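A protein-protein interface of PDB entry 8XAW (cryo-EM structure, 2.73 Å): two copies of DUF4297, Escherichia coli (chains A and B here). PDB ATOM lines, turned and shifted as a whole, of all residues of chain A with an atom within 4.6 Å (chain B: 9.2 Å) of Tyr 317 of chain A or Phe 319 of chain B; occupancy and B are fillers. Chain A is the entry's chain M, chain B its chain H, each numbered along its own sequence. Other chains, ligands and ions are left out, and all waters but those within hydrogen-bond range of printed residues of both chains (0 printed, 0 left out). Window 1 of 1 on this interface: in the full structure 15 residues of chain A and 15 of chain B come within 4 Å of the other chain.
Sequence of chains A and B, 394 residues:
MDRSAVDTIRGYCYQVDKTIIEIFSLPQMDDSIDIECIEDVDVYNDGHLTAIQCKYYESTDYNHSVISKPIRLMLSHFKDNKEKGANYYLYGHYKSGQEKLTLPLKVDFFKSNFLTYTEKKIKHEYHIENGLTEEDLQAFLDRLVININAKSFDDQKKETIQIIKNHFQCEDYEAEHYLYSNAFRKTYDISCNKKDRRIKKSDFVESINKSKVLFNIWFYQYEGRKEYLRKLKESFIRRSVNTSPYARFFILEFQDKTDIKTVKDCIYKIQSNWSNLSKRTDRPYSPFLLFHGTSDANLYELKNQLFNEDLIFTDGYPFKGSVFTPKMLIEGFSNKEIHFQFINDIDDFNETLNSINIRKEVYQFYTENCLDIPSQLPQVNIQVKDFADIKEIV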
ATOM      1  N   LYS A 303     -22.158   8.534  23.853  1.00  0.00           N
ATOM      2  CA  LYS A 303     -20.802   8.982  24.157  1.00  0.00           C
ATOM      3  C   LYS A 303     -20.747   9.732  25.482  1.00  0.00           C
ATOM      4  O   LYS A 303     -19.775   9.603  26.234  1.00  0.00           O
ATOM      5  CB  LYS A 303     -20.279   9.858  23.021  1.00  0.00           C
ATOM      6  CG  LYS A 303     -20.320   9.176  21.668  1.00  0.00           C
ATOM      7  CD  LYS A 303     -19.759  10.039  20.550  1.00  0.00           C
ATOM      8  CE  LYS A 303     -18.513  10.788  20.947  1.00  0.00           C
ATOM      9  NZ  LYS A 303     -17.936  11.470  19.764  1.00  0.00           N
ATOM     10  N   ASN A 304     -21.774  10.531  25.777  1.00  0.00           N
ATOM     11  CA  ASN A 304     -21.825  11.233  27.055  1.00  0.00           C
ATOM     12  C   ASN A 304     -22.034  10.267  28.212  1.00  0.00           C
ATOM     13  O   ASN A 304     -21.503  10.482  29.308  1.00  0.00           O
ATOM     14  CB  ASN A 304     -22.928  12.288  27.033  1.00  0.00           C
ATOM     15  CG  ASN A 304     -22.454  13.608  26.475  1.00  0.00           C
ATOM     16  OD1 ASN A 304     -21.689  14.324  27.120  1.00  0.00           O
ATOM     17  ND2 ASN A 304     -22.902  13.939  25.271  1.00  0.00           N
ATOM     18  N   PHE A 307     -18.652   8.479  29.018  1.00  0.00           N
ATOM     19  CA  PHE A 307     -17.636   9.308  29.659  1.00  0.00           C
ATOM     20  C   PHE A 307     -17.882   9.463  31.154  1.00  0.00           C
ATOM     21  O   PHE A 307     -16.925   9.580  31.927  1.00  0.00           O
ATOM     22  CB  PHE A 307     -17.577  10.679  28.989  1.00  0.00           C
ATOM     23  CG  PHE A 307     -16.220  11.316  29.039  1.00  0.00           C
ATOM     24  CD1 PHE A 307     -15.257  11.001  28.094  1.00  0.00           C
ATOM     25  CD2 PHE A 307     -15.906  12.227  30.033  1.00  0.00           C
ATOM     26  CE1 PHE A 307     -14.008  11.588  28.137  1.00  0.00           C
ATOM     27  CE2 PHE A 307     -14.658  12.815  30.084  1.00  0.00           C
ATOM     28  CZ  PHE A 307     -13.707  12.495  29.136  1.00  0.00           C
ATOM     29  N   PHE A 313     -12.457   7.651  26.300  1.00  0.00           N
ATOM     30  CA  PHE A 313     -12.229   7.426  24.881  1.00  0.00           C
ATOM     31  C   PHE A 313     -11.775   8.727  24.229  1.00  0.00           C
ATOM     32  O   PHE A 313     -11.648   9.768  24.879  1.00  0.00           O
ATOM     33  CB  PHE A 313     -13.484   6.865  24.190  1.00  0.00           C
ATOM     34  CG  PHE A 313     -14.715   7.723  24.344  1.00  0.00           C
ATOM     35  CD1 PHE A 313     -15.004   8.724  23.429  1.00  0.00           C
ATOM     36  CD2 PHE A 313     -15.595   7.514  25.394  1.00  0.00           C
ATOM     37  CE1 PHE A 313     -16.131   9.507  23.567  1.00  0.00           C
ATOM     38  CE2 PHE A 313     -16.725   8.293  25.536  1.00  0.00           C
ATOM     39  CZ  PHE A 313     -16.993   9.289  24.621  1.00  0.00           C
ATOM     40  N   ASP A 315     -11.934  10.744  20.023  1.00  0.00           N
ATOM     41  CA  ASP A 315     -12.425  10.665  18.652  1.00  0.00           C
ATOM     42  C   ASP A 315     -11.789  11.704  17.737  1.00  0.00           C
ATOM     43  O   ASP A 315     -12.383  12.052  16.710  1.00  0.00           O
ATOM     44  CB  ASP A 315     -13.941  10.827  18.595  1.00  0.00           C
ATOM     45  CG  ASP A 315     -14.452  11.853  19.575  1.00  0.00           C
ATOM     46  OD1 ASP A 315     -13.628  12.553  20.198  1.00  0.00           O
ATOM     47  OD2 ASP A 315     -15.683  11.971  19.705  1.00  0.00           O
ATOM     48  N   GLY A 316     -10.610  12.216  18.075  1.00  0.00           N
ATOM     49  CA  GLY A 316      -9.979  13.214  17.241  1.00  0.00           C
ATOM     50  C   GLY A 316     -10.553  14.605  17.357  1.00  0.00           C
ATOM     51  O   GLY A 316     -10.225  15.464  16.531  1.00  0.00           O
ATOM     52  N   TYR A 317     -11.401  14.855  18.350  1.00  0.00           N
ATOM     53  CA  TYR A 317     -11.975  16.177  18.603  1.00  0.00           C
ATOM     54  C   TYR A 317     -11.677  16.541  20.050  1.00  0.00           C
ATOM     55  O   TYR A 317     -12.547  16.426  20.924  1.00  0.00           O
ATOM     56  CB  TYR A 317     -13.477  16.193  18.319  1.00  0.00           C
ATOM     57  CG  TYR A 317     -13.837  15.846  16.893  1.00  0.00           C
ATOM     58  CD1 TYR A 317     -13.680  16.773  15.872  1.00  0.00           C
ATOM     59  CD2 TYR A 317     -14.322  14.588  16.568  1.00  0.00           C
ATOM     60  CE1 TYR A 317     -14.006  16.460  14.568  1.00  0.00           C
ATOM     61  CE2 TYR A 317     -14.648  14.264  15.265  1.00  0.00           C
ATOM     62  CZ  TYR A 317     -14.489  15.204  14.271  1.00  0.00           C
ATOM     63  OH  TYR A 317     -14.814  14.886  12.973  1.00  0.00           O
ATOM     64  N   PRO A 318     -10.446  16.978  20.341  1.00  0.00           N
ATOM     65  CA  PRO A 318     -10.073  17.249  21.740  1.00  0.00           C
ATOM     66  C   PRO A 318     -10.760  18.461  22.342  1.00  0.00           C
ATOM     67  O   PRO A 318     -10.803  18.573  23.574  1.00  0.00           O
ATOM     68  CB  PRO A 318      -8.556  17.454  21.659  1.00  0.00           C
ATOM     69  CG  PRO A 318      -8.327  17.937  20.269  1.00  0.00           C
ATOM     70  CD  PRO A 318      -9.333  17.235  19.412  1.00  0.00           C
ATOM     71  N   PHE A 319     -11.291  19.369  21.529  1.00  0.00           N
ATOM     72  CA  PHE A 319     -11.974  20.553  22.028  1.00  0.00           C
ATOM     73  C   PHE A 319     -13.147  20.871  21.113  1.00  0.00           C
ATOM     74  O   PHE A 319     -13.302  20.283  20.040  1.00  0.00           O
ATOM     75  CB  PHE A 319     -11.019  21.753  22.150  1.00  0.00           C
ATOM     76  CG  PHE A 319     -10.218  22.037  20.908  1.00  0.00           C
ATOM     77  CD1 PHE A 319      -8.970  21.464  20.726  1.00  0.00           C
ATOM     78  CD2 PHE A 319     -10.700  22.897  19.934  1.00  0.00           C
ATOM     79  CE1 PHE A 319      -8.229  21.726  19.592  1.00  0.00           C
ATOM     80  CE2 PHE A 319      -9.963  23.163  18.799  1.00  0.00           C
ATOM     81  CZ  PHE A 319      -8.727  22.577  18.629  1.00  0.00           C
ATOM     82  N   SER A 322     -13.315  21.731  16.776  1.00  0.00           N
ATOM     83  CA  SER A 322     -12.036  21.212  16.321  1.00  0.00           C
ATOM     84  C   SER A 322     -12.203  20.452  15.013  1.00  0.00           C
ATOM     85  O   SER A 322     -13.232  19.819  14.765  1.00  0.00           O
ATOM     86  CB  SER A 322     -11.414  20.287  17.367  1.00  0.00           C
ATOM     87  OG  SER A 322     -10.674  19.250  16.750  1.00  0.00           O
ATOM     88  N   VAL A 323     -11.173  20.529  14.171  1.00  0.00           N
ATOM     89  CA  VAL A 323     -11.100  19.631  13.031  1.00  0.00           C
ATOM     90  C   VAL A 323     -10.771  18.224  13.519  1.00  0.00           C
ATOM     91  O   VAL A 323     -10.351  18.010  14.663  1.00  0.00           O
ATOM     92  CB  VAL A 323     -10.066  20.123  12.006  1.00  0.00           C
ATOM     93  CG1 VAL A 323     -10.301  21.590  11.679  1.00  0.00           C
ATOM     94  CG2 VAL A 323      -8.656  19.913  12.532  1.00  0.00           C
ATOM     95  N   PHE A 324     -10.988  17.246  12.644  1.00  0.00           N
ATOM     96  CA  PHE A 324     -10.624  15.875  12.974  1.00  0.00           C
ATOM     97  C   PHE A 324      -9.111  15.753  13.059  1.00  0.00           C
ATOM     98  O   PHE A 324      -8.405  15.966  12.068  1.00  0.00           O
ATOM     99  CB  PHE A 324     -11.182  14.898  11.946  1.00  0.00           C
ATOM    100  CG  PHE A 324     -10.948  13.458  12.301  1.00  0.00           C
ATOM    101  CD1 PHE A 324     -11.329  12.965  13.536  1.00  0.00           C
ATOM    102  CD2 PHE A 324     -10.326  12.602  11.408  1.00  0.00           C
ATOM    103  CE1 PHE A 324     -11.103  11.643  13.869  1.00  0.00           C
ATOM    104  CE2 PHE A 324     -10.100  11.279  11.736  1.00  0.00           C
ATOM    105  CZ  PHE A 324     -10.489  10.801  12.968  1.00  0.00           C
ATOM    106  N   ASN A 344     -16.595   8.922  14.660  1.00  0.00           N
ATOM    107  CA  ASN A 344     -17.929   9.503  14.547  1.00  0.00           C
ATOM    108  C   ASN A 344     -18.689   8.948  13.347  1.00  0.00           C
ATOM    109  O   ASN A 344     -19.840   8.515  13.482  1.00  0.00           O
ATOM    110  CB  ASN A 344     -17.826  11.026  14.463  1.00  0.00           C
ATOM    111  CG  ASN A 344     -18.114  11.702  15.787  1.00  0.00           C
ATOM    112  OD1 ASN A 344     -17.331  11.601  16.732  1.00  0.00           O
ATOM    113  ND2 ASN A 344     -19.244  12.394  15.865  1.00  0.00           N
ATOM    114  N   ASP A 348     -14.346  10.404   9.027  1.00  0.00           N
ATOM    115  CA  ASP A 348     -13.262  10.236   9.985  1.00  0.00           C
ATOM    116  C   ASP A 348     -12.720   8.814  10.012  1.00  0.00           C
ATOM    117  O   ASP A 348     -11.566   8.615  10.405  1.00  0.00           O
ATOM    118  CB  ASP A 348     -13.724  10.647  11.383  1.00  0.00           C
ATOM    119  CG  ASP A 348     -14.614  11.871  11.364  1.00  0.00           C
ATOM    120  OD1 ASP A 348     -14.428  12.726  10.474  1.00  0.00           O
ATOM    121  OD2 ASP A 348     -15.491  11.985  12.244  1.00  0.00           O
ATOM    122  N   ASN B 304      -7.752  25.956  17.092  1.00  0.00           N
ATOM    123  CA  ASN B 304      -7.176  24.960  16.195  1.00  0.00           C
ATOM    124  C   ASN B 304      -5.692  25.209  15.963  1.00  0.00           C
ATOM    125  O   ASN B 304      -4.904  24.258  15.909  1.00  0.00           O
ATOM    126  CB  ASN B 304      -7.936  24.944  14.870  1.00  0.00           C
ATOM    127  CG  ASN B 304      -9.144  24.031  14.907  1.00  0.00           C
ATOM    128  OD1 ASN B 304      -9.018  22.826  15.115  1.00  0.00           O
ATOM    129  ND2 ASN B 304     -10.325  24.603  14.708  1.00  0.00           N
ATOM    130  N   PHE B 307      -3.495  24.108  18.982  1.00  0.00           N
ATOM    131  CA  PHE B 307      -3.287  22.673  19.128  1.00  0.00           C
ATOM    132  C   PHE B 307      -2.234  22.152  18.156  1.00  0.00           C
ATOM    133  O   PHE B 307      -1.501  21.214  18.487  1.00  0.00           O
ATOM    134  CB  PHE B 307      -4.607  21.930  18.936  1.00  0.00           C
ATOM    135  CG  PHE B 307      -4.740  20.711  19.798  1.00  0.00           C
ATOM    136  CD1 PHE B 307      -5.162  20.820  21.114  1.00  0.00           C
ATOM    137  CD2 PHE B 307      -4.431  19.459  19.298  1.00  0.00           C
ATOM    138  CE1 PHE B 307      -5.281  19.700  21.913  1.00  0.00           C
ATOM    139  CE2 PHE B 307      -4.544  18.338  20.090  1.00  0.00           C
ATOM    140  CZ  PHE B 307      -4.970  18.457  21.400  1.00  0.00           C
ATOM    141  N   PHE B 313      -4.460  22.176  25.434  1.00  0.00           N
ATOM    142  CA  PHE B 313      -5.376  22.787  26.382  1.00  0.00           C
ATOM    143  C   PHE B 313      -6.612  21.908  26.526  1.00  0.00           C
ATOM    144  O   PHE B 313      -6.764  20.890  25.845  1.00  0.00           O
ATOM    145  CB  PHE B 313      -5.758  24.211  25.949  1.00  0.00           C
ATOM    146  CG  PHE B 313      -6.397  24.292  24.588  1.00  0.00           C
ATOM    147  CD1 PHE B 313      -5.619  24.430  23.449  1.00  0.00           C
ATOM    148  CD2 PHE B 313      -7.777  24.252  24.449  1.00  0.00           C
ATOM    149  CE1 PHE B 313      -6.201  24.507  22.202  1.00  0.00           C
ATOM    150  CE2 PHE B 313      -8.362  24.328  23.203  1.00  0.00           C
ATOM    151  CZ  PHE B 313      -7.573  24.458  22.079  1.00  0.00           C
ATOM    152  N   THR B 314      -7.501  22.313  27.428  1.00  0.00           N
ATOM    153  CA  THR B 314      -8.795  21.674  27.598  1.00  0.00           C
ATOM    154  C   THR B 314      -9.867  22.750  27.669  1.00  0.00           C
ATOM    155  O   THR B 314      -9.610  23.877  28.102  1.00  0.00           O
ATOM    156  CB  THR B 314      -8.845  20.801  28.861  1.00  0.00           C
ATOM    157  OG1 THR B 314     -10.206  20.477  29.167  1.00  0.00           O
ATOM    158  CG2 THR B 314      -8.237  21.535  30.041  1.00  0.00           C
ATOM    159  N   ASP B 315     -11.075  22.398  27.230  1.00  0.00           N
ATOM    160  CA  ASP B 315     -12.196  23.326  27.247  1.00  0.00           C
ATOM    161  C   ASP B 315     -13.433  22.738  27.913  1.00  0.00           C
ATOM    162  O   ASP B 315     -14.487  23.382  27.912  1.00  0.00           O
ATOM    163  CB  ASP B 315     -12.546  23.778  25.825  1.00  0.00           C
ATOM    164  CG  ASP B 315     -12.937  22.626  24.929  1.00  0.00           C
ATOM    165  OD1 ASP B 315     -12.536  21.480  25.221  1.00  0.00           O
ATOM    166  OD2 ASP B 315     -13.647  22.863  23.931  1.00  0.00           O
ATOM    167  N   GLY B 316     -13.333  21.541  28.482  1.00  0.00           N
ATOM    168  CA  GLY B 316     -14.499  20.866  29.005  1.00  0.00           C
ATOM    169  C   GLY B 316     -15.310  20.119  27.973  1.00  0.00           C
ATOM    170  O   GLY B 316     -16.385  19.610  28.305  1.00  0.00           O
ATOM    171  N   TYR B 317     -14.830  20.036  26.733  1.00  0.00           N
ATOM    172  CA  TYR B 317     -15.512  19.319  25.655  1.00  0.00           C
ATOM    173  C   TYR B 317     -14.536  18.318  25.053  1.00  0.00           C
ATOM    174  O   TYR B 317     -13.894  18.595  24.032  1.00  0.00           O
ATOM    175  CB  TYR B 317     -16.047  20.269  24.582  1.00  0.00           C
ATOM    176  CG  TYR B 317     -17.084  21.264  25.056  1.00  0.00           C
ATOM    177  CD1 TYR B 317     -16.721  22.399  25.771  1.00  0.00           C
ATOM    178  CD2 TYR B 317     -18.432  21.063  24.789  1.00  0.00           C
ATOM    179  CE1 TYR B 317     -17.667  23.302  26.201  1.00  0.00           C
ATOM    180  CE2 TYR B 317     -19.386  21.963  25.217  1.00  0.00           C
ATOM    181  CZ  TYR B 317     -18.999  23.081  25.923  1.00  0.00           C
ATOM    182  OH  TYR B 317     -19.947  23.979  26.350  1.00  0.00           O
ATOM    183  N   PRO B 318     -14.397  17.139  25.665  1.00  0.00           N
ATOM    184  CA  PRO B 318     -13.448  16.146  25.138  1.00  0.00           C
ATOM    185  C   PRO B 318     -13.916  15.445  23.870  1.00  0.00           C
ATOM    186  O   PRO B 318     -13.108  14.742  23.250  1.00  0.00           O
ATOM    187  CB  PRO B 318     -13.304  15.151  26.296  1.00  0.00           C
ATOM    188  CG  PRO B 318     -14.561  15.292  27.074  1.00  0.00           C
ATOM    189  CD  PRO B 318     -15.008  16.710  26.935  1.00  0.00           C
ATOM    190  N   PHE B 319     -15.174  15.608  23.464  1.00  0.00           N
ATOM    191  CA  PHE B 319     -15.676  14.955  22.262  1.00  0.00           C
ATOM    192  C   PHE B 319     -16.866  15.745  21.734  1.00  0.00           C
ATOM    193  O   PHE B 319     -17.407  16.618  22.416  1.00  0.00           O
ATOM    194  CB  PHE B 319     -16.051  13.488  22.525  1.00  0.00           C
ATOM    195  CG  PHE B 319     -16.979  13.277  23.695  1.00  0.00           C
ATOM    196  CD1 PHE B 319     -16.480  13.097  24.974  1.00  0.00           C
ATOM    197  CD2 PHE B 319     -18.350  13.216  23.504  1.00  0.00           C
ATOM    198  CE1 PHE B 319     -17.331  12.894  26.041  1.00  0.00           C
ATOM    199  CE2 PHE B 319     -19.203  13.001  24.565  1.00  0.00           C
ATOM    200  CZ  PHE B 319     -18.693  12.844  25.837  1.00  0.00           C
ATOM    201  N   LYS B 320     -17.251  15.444  20.493  1.00  0.00           N
ATOM    202  CA  LYS B 320     -18.422  16.079  19.900  1.00  0.00           C
ATOM    203  C   LYS B 320     -19.697  15.640  20.604  1.00  0.00           C
ATOM    204  O   LYS B 320     -19.863  14.468  20.956  1.00  0.00           O
ATOM    205  CB  LYS B 320     -18.527  15.756  18.412  1.00  0.00           C
ATOM    206  CG  LYS B 320     -17.347  16.185  17.578  1.00  0.00           C
ATOM    207  CD  LYS B 320     -17.676  16.047  16.103  1.00  0.00           C
ATOM    208  CE  LYS B 320     -18.468  17.244  15.605  1.00  0.00           C
ATOM    209  NZ  LYS B 320     -17.930  17.780  14.327  1.00  0.00           N
ATOM    210  N   GLY B 321     -20.603  16.592  20.807  1.00  0.00           N
ATOM    211  CA  GLY B 321     -21.839  16.325  21.502  1.00  0.00           C
ATOM    212  C   GLY B 321     -21.716  16.245  23.003  1.00  0.00           C
ATOM    213  O   GLY B 321     -22.709  15.937  23.674  1.00  0.00           O
ATOM    214  N   SER B 322     -20.533  16.501  23.550  1.00  0.00           N
ATOM    215  CA  SER B 322     -20.345  16.451  24.990  1.00  0.00           C
ATOM    216  C   SER B 322     -21.005  17.650  25.649  1.00  0.00           C
ATOM    217  O   SER B 322     -20.893  18.780  25.164  1.00  0.00           O
ATOM    218  CB  SER B 322     -18.856  16.426  25.331  1.00  0.00           C
ATOM    219  OG  SER B 322     -18.393  17.719  25.664  1.00  0.00           O
ATOM    220  N   VAL B 323     -21.706  17.401  26.754  1.00  0.00           N
ATOM    221  CA  VAL B 323     -22.083  18.491  27.636  1.00  0.00           C
ATOM    222  C   VAL B 323     -20.819  19.057  28.271  1.00  0.00           C
ATOM    223  O   VAL B 323     -19.791  18.374  28.378  1.00  0.00           O
ATOM    224  CB  VAL B 323     -23.088  18.019  28.703  1.00  0.00           C
ATOM    225  CG1 VAL B 323     -24.391  17.591  28.047  1.00  0.00           C
ATOM    226  CG2 VAL B 323     -22.505  16.877  29.516  1.00  0.00           C
ATOM    227  N   PHE B 324     -20.874  20.327  28.659  1.00  0.00           N
ATOM    228  CA  PHE B 324     -19.708  20.965  29.256  1.00  0.00           C
ATOM    229  C   PHE B 324     -19.454  20.372  30.636  1.00  0.00           C
ATOM    230  O   PHE B 324     -20.316  20.440  31.517  1.00  0.00           O
ATOM    231  CB  PHE B 324     -19.911  22.472  29.351  1.00  0.00           C
ATOM    232  CG  PHE B 324     -18.921  23.152  30.247  1.00  0.00           C
ATOM    233  CD1 PHE B 324     -17.578  23.175  29.914  1.00  0.00           C
ATOM    234  CD2 PHE B 324     -19.325  23.746  31.431  1.00  0.00           C
ATOM    235  CE1 PHE B 324     -16.659  23.789  30.733  1.00  0.00           C
ATOM    236  CE2 PHE B 324     -18.406  24.362  32.258  1.00  0.00           C
ATOM    237  CZ  PHE B 324     -17.072  24.383  31.908  1.00  0.00           C
ATOM    238  N   THR B 325     -18.274  19.778  30.818  1.00  0.00           N
ATOM    239  CA  THR B 325     -17.899  19.200  32.098  1.00  0.00           C
ATOM    240  C   THR B 325     -16.900  20.118  32.779  1.00  0.00           C
ATOM    241  O   THR B 325     -15.818  20.358  32.219  1.00  0.00           O
ATOM    242  CB  THR B 325     -17.299  17.806  31.923  1.00  0.00           C
ATOM    243  OG1 THR B 325     -15.889  17.924  31.719  1.00  0.00           O
ATOM    244  CG2 THR B 325     -17.916  17.093  30.736  1.00  0.00           C
ATOM    245  N   MET B 328     -13.098  18.333  33.766  1.00  0.00           N
ATOM    246  CA  MET B 328     -11.943  18.283  32.871  1.00  0.00           C
ATOM    247  C   MET B 328     -11.076  19.529  32.998  1.00  0.00           C
ATOM    248  O   MET B 328      -9.848  19.438  32.882  1.00  0.00           O
ATOM    249  CB  MET B 328     -12.394  18.099  31.418  1.00  0.00           C
ATOM    250  CG  MET B 328     -13.001  16.734  31.061  1.00  0.00           C
ATOM    251  SD  MET B 328     -11.811  15.442  30.619  1.00  0.00           S
ATOM    252  CE  MET B 328     -11.400  14.717  32.201  1.00  0.00           C
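Asn 304 of chain A touches Phe 319 of chain B, and with the chains exchanged Phe 319 of chain A touches Asn 304 of chain B.
Asn 304 of chain A touches Val 323 of chain B, and with the chains exchanged Val 323 of chain A touches Asn 304 of chain B.
Phe 307 of chain A touches Pro 318 of chain B, and with the chains exchanged Pro 318 of chain A touches Phe 307 of chain B.
Phe 307 of chain A touches Phe 319 of chain B, and with the chains exchanged Phe 319 of chain A touches Phe 307 of chain B.
Positions printed for both chains: 304, 307, 313, 315, 316, 317, 318, 319, 322, 323 and 324.
Tyr 317 of chain A touches three residues of chain B.
Phe 319 of chain B touches just these residues of chain A: Lys 303 (3.4 Å), Asn 304 (3.6 Å), Phe 307 (3.5 Å), Phe 313 (3.9 Å), Asp 315 (3.2 Å) and Tyr 317 (3.7 Å).
No residue of chain B comes within 4 Å of Gly 316 of chain A.
Pro 318 of chain A touches just these residues of chain B: Phe 307, Asp 315, Tyr 317 and Pro 318.
Ser 322 of chain A touches just one residue of chain B: Asn 304 (3.6 Å).
Of the printed residues of chain A, Asn 304 of chain B touches Phe 319, Ser 322 and Val 323.
Of the printed residues of chain A, Pro 318 of chain B touches Phe 307, Asp 315, Tyr 317 and Pro 318.
Printed residues of chain B within 4 Å of Phe 319 of chain A: Asn 304, Phe 307, Phe 313, Asp 315 and Tyr 317.
Printed residues of chain A within 4 Å of Val 323 of chain B: Asn 304 (3.1 Å).
Of the printed residues of chain B, Phe 313 of chain A touches Phe 319.
The nearest printed residue of chain A that does not touch Val 323 of chain B is Phe 307 of chain A (7.5 Å).
Lys 303 of chain A touches Lys 320 of chain B (NZ to O, 3.8 Å).
Asn 304 of chain A touches Ser 322 of chain B.
Met 328 of chain B touches Phe 307 of chain A.
Phe 313 of chain A touches Phe 319 of chain B.
Asp 315 of chain A touches Phe 319 of chain B.
Phe 319 of chain B touches Tyr 317 of chain A (CA to O, 3.7 Å).
CD2 of Tyr 317 of chain A touches CG of Lys 320 of chain B (3.6 Å).
Phe 307 of chain B touches Phe 319 of chain A.
Phe 319 of chain A touches Phe 313 of chain B (CD1 to CZ, 3.6 Å).
CA of Ser 322 of chain A touches OD1 of Asn 304 of chain B (3.6 Å).
Of the 16 printed residues of chain B, 12 touch a printed residue of chain A.
Printed residues of chain B that touch a printed residue of chain A: Asn 304, Phe 307, Phe 313, Asp 315, Tyr 317, Pro 318, Phe 319, Lys 320, Gly 321, Ser 322, Val 323 and Met 328.
Hydrophobic or aromatic side chains of chain B that line the printed part of chain A: Phe 307, Phe 313, Pro 318, Phe 319, Val 323 and Met 328.
Hydrophobic or aromatic side chains of chain A within 4 Å of the printed part of chain B: Phe 307, Phe 313, Tyr 317, Pro 318, Phe 319 and Val 323.
Among the printed residues, 28 pairs touch across the chains.
Among the printed residues, no Asp or Glu carboxylate lies within 4 Å of a Lys or Arg side-chain nitrogen of the other chain.
The backbone NH (N) of Tyr 317 of chain B sits at hydrogen-bond distance from the side-chain carboxylate (OD1) of Asp 315 of chain B (3.1 Å).
N of Met 328 of chain B sits close to OG1 of Thr 325 of chain B, at 3.5 Å.
The side-chain amide oxygen (OD1) of Asn 344 of chain A sits at hydrogen-bond distance from the side-chain amino group (NZ) of Lys 303 of chain A, at 3.1 Å.
OD1 of Asn 344 of chain A lies close to OD2 of Asp 315 of chain A (3.4 Å).
OH of Tyr 317 of chain A lies within hydrogen-bond range of OD2 of Asp 348 of chain A (3.1 Å).
OD1 of Asn 304 of chain B sits at hydrogen-bond distance from N of Val 323 of chain A (3.3 Å).
The backbone carbonyl oxygen (O) of Gly 321 of chain B sits at hydrogen-bond distance from the side-chain amide nitrogen (ND2) of Asn 304 of chain A (2.6 Å).
The backbone NH of Val 323 of chain B is in hydrogen-bond range of the side-chain amide oxygen of Asn 304 of chain A (3.1 Å).
The backbone carbonyl oxygen (O) of Tyr 317 of chain A sits close to the backbone carbonyl oxygen (O) of Pro 318 of chain B, at 2.9 Å.
O of Pro 318 of chain A lies close to O of Tyr 317 of chain B.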
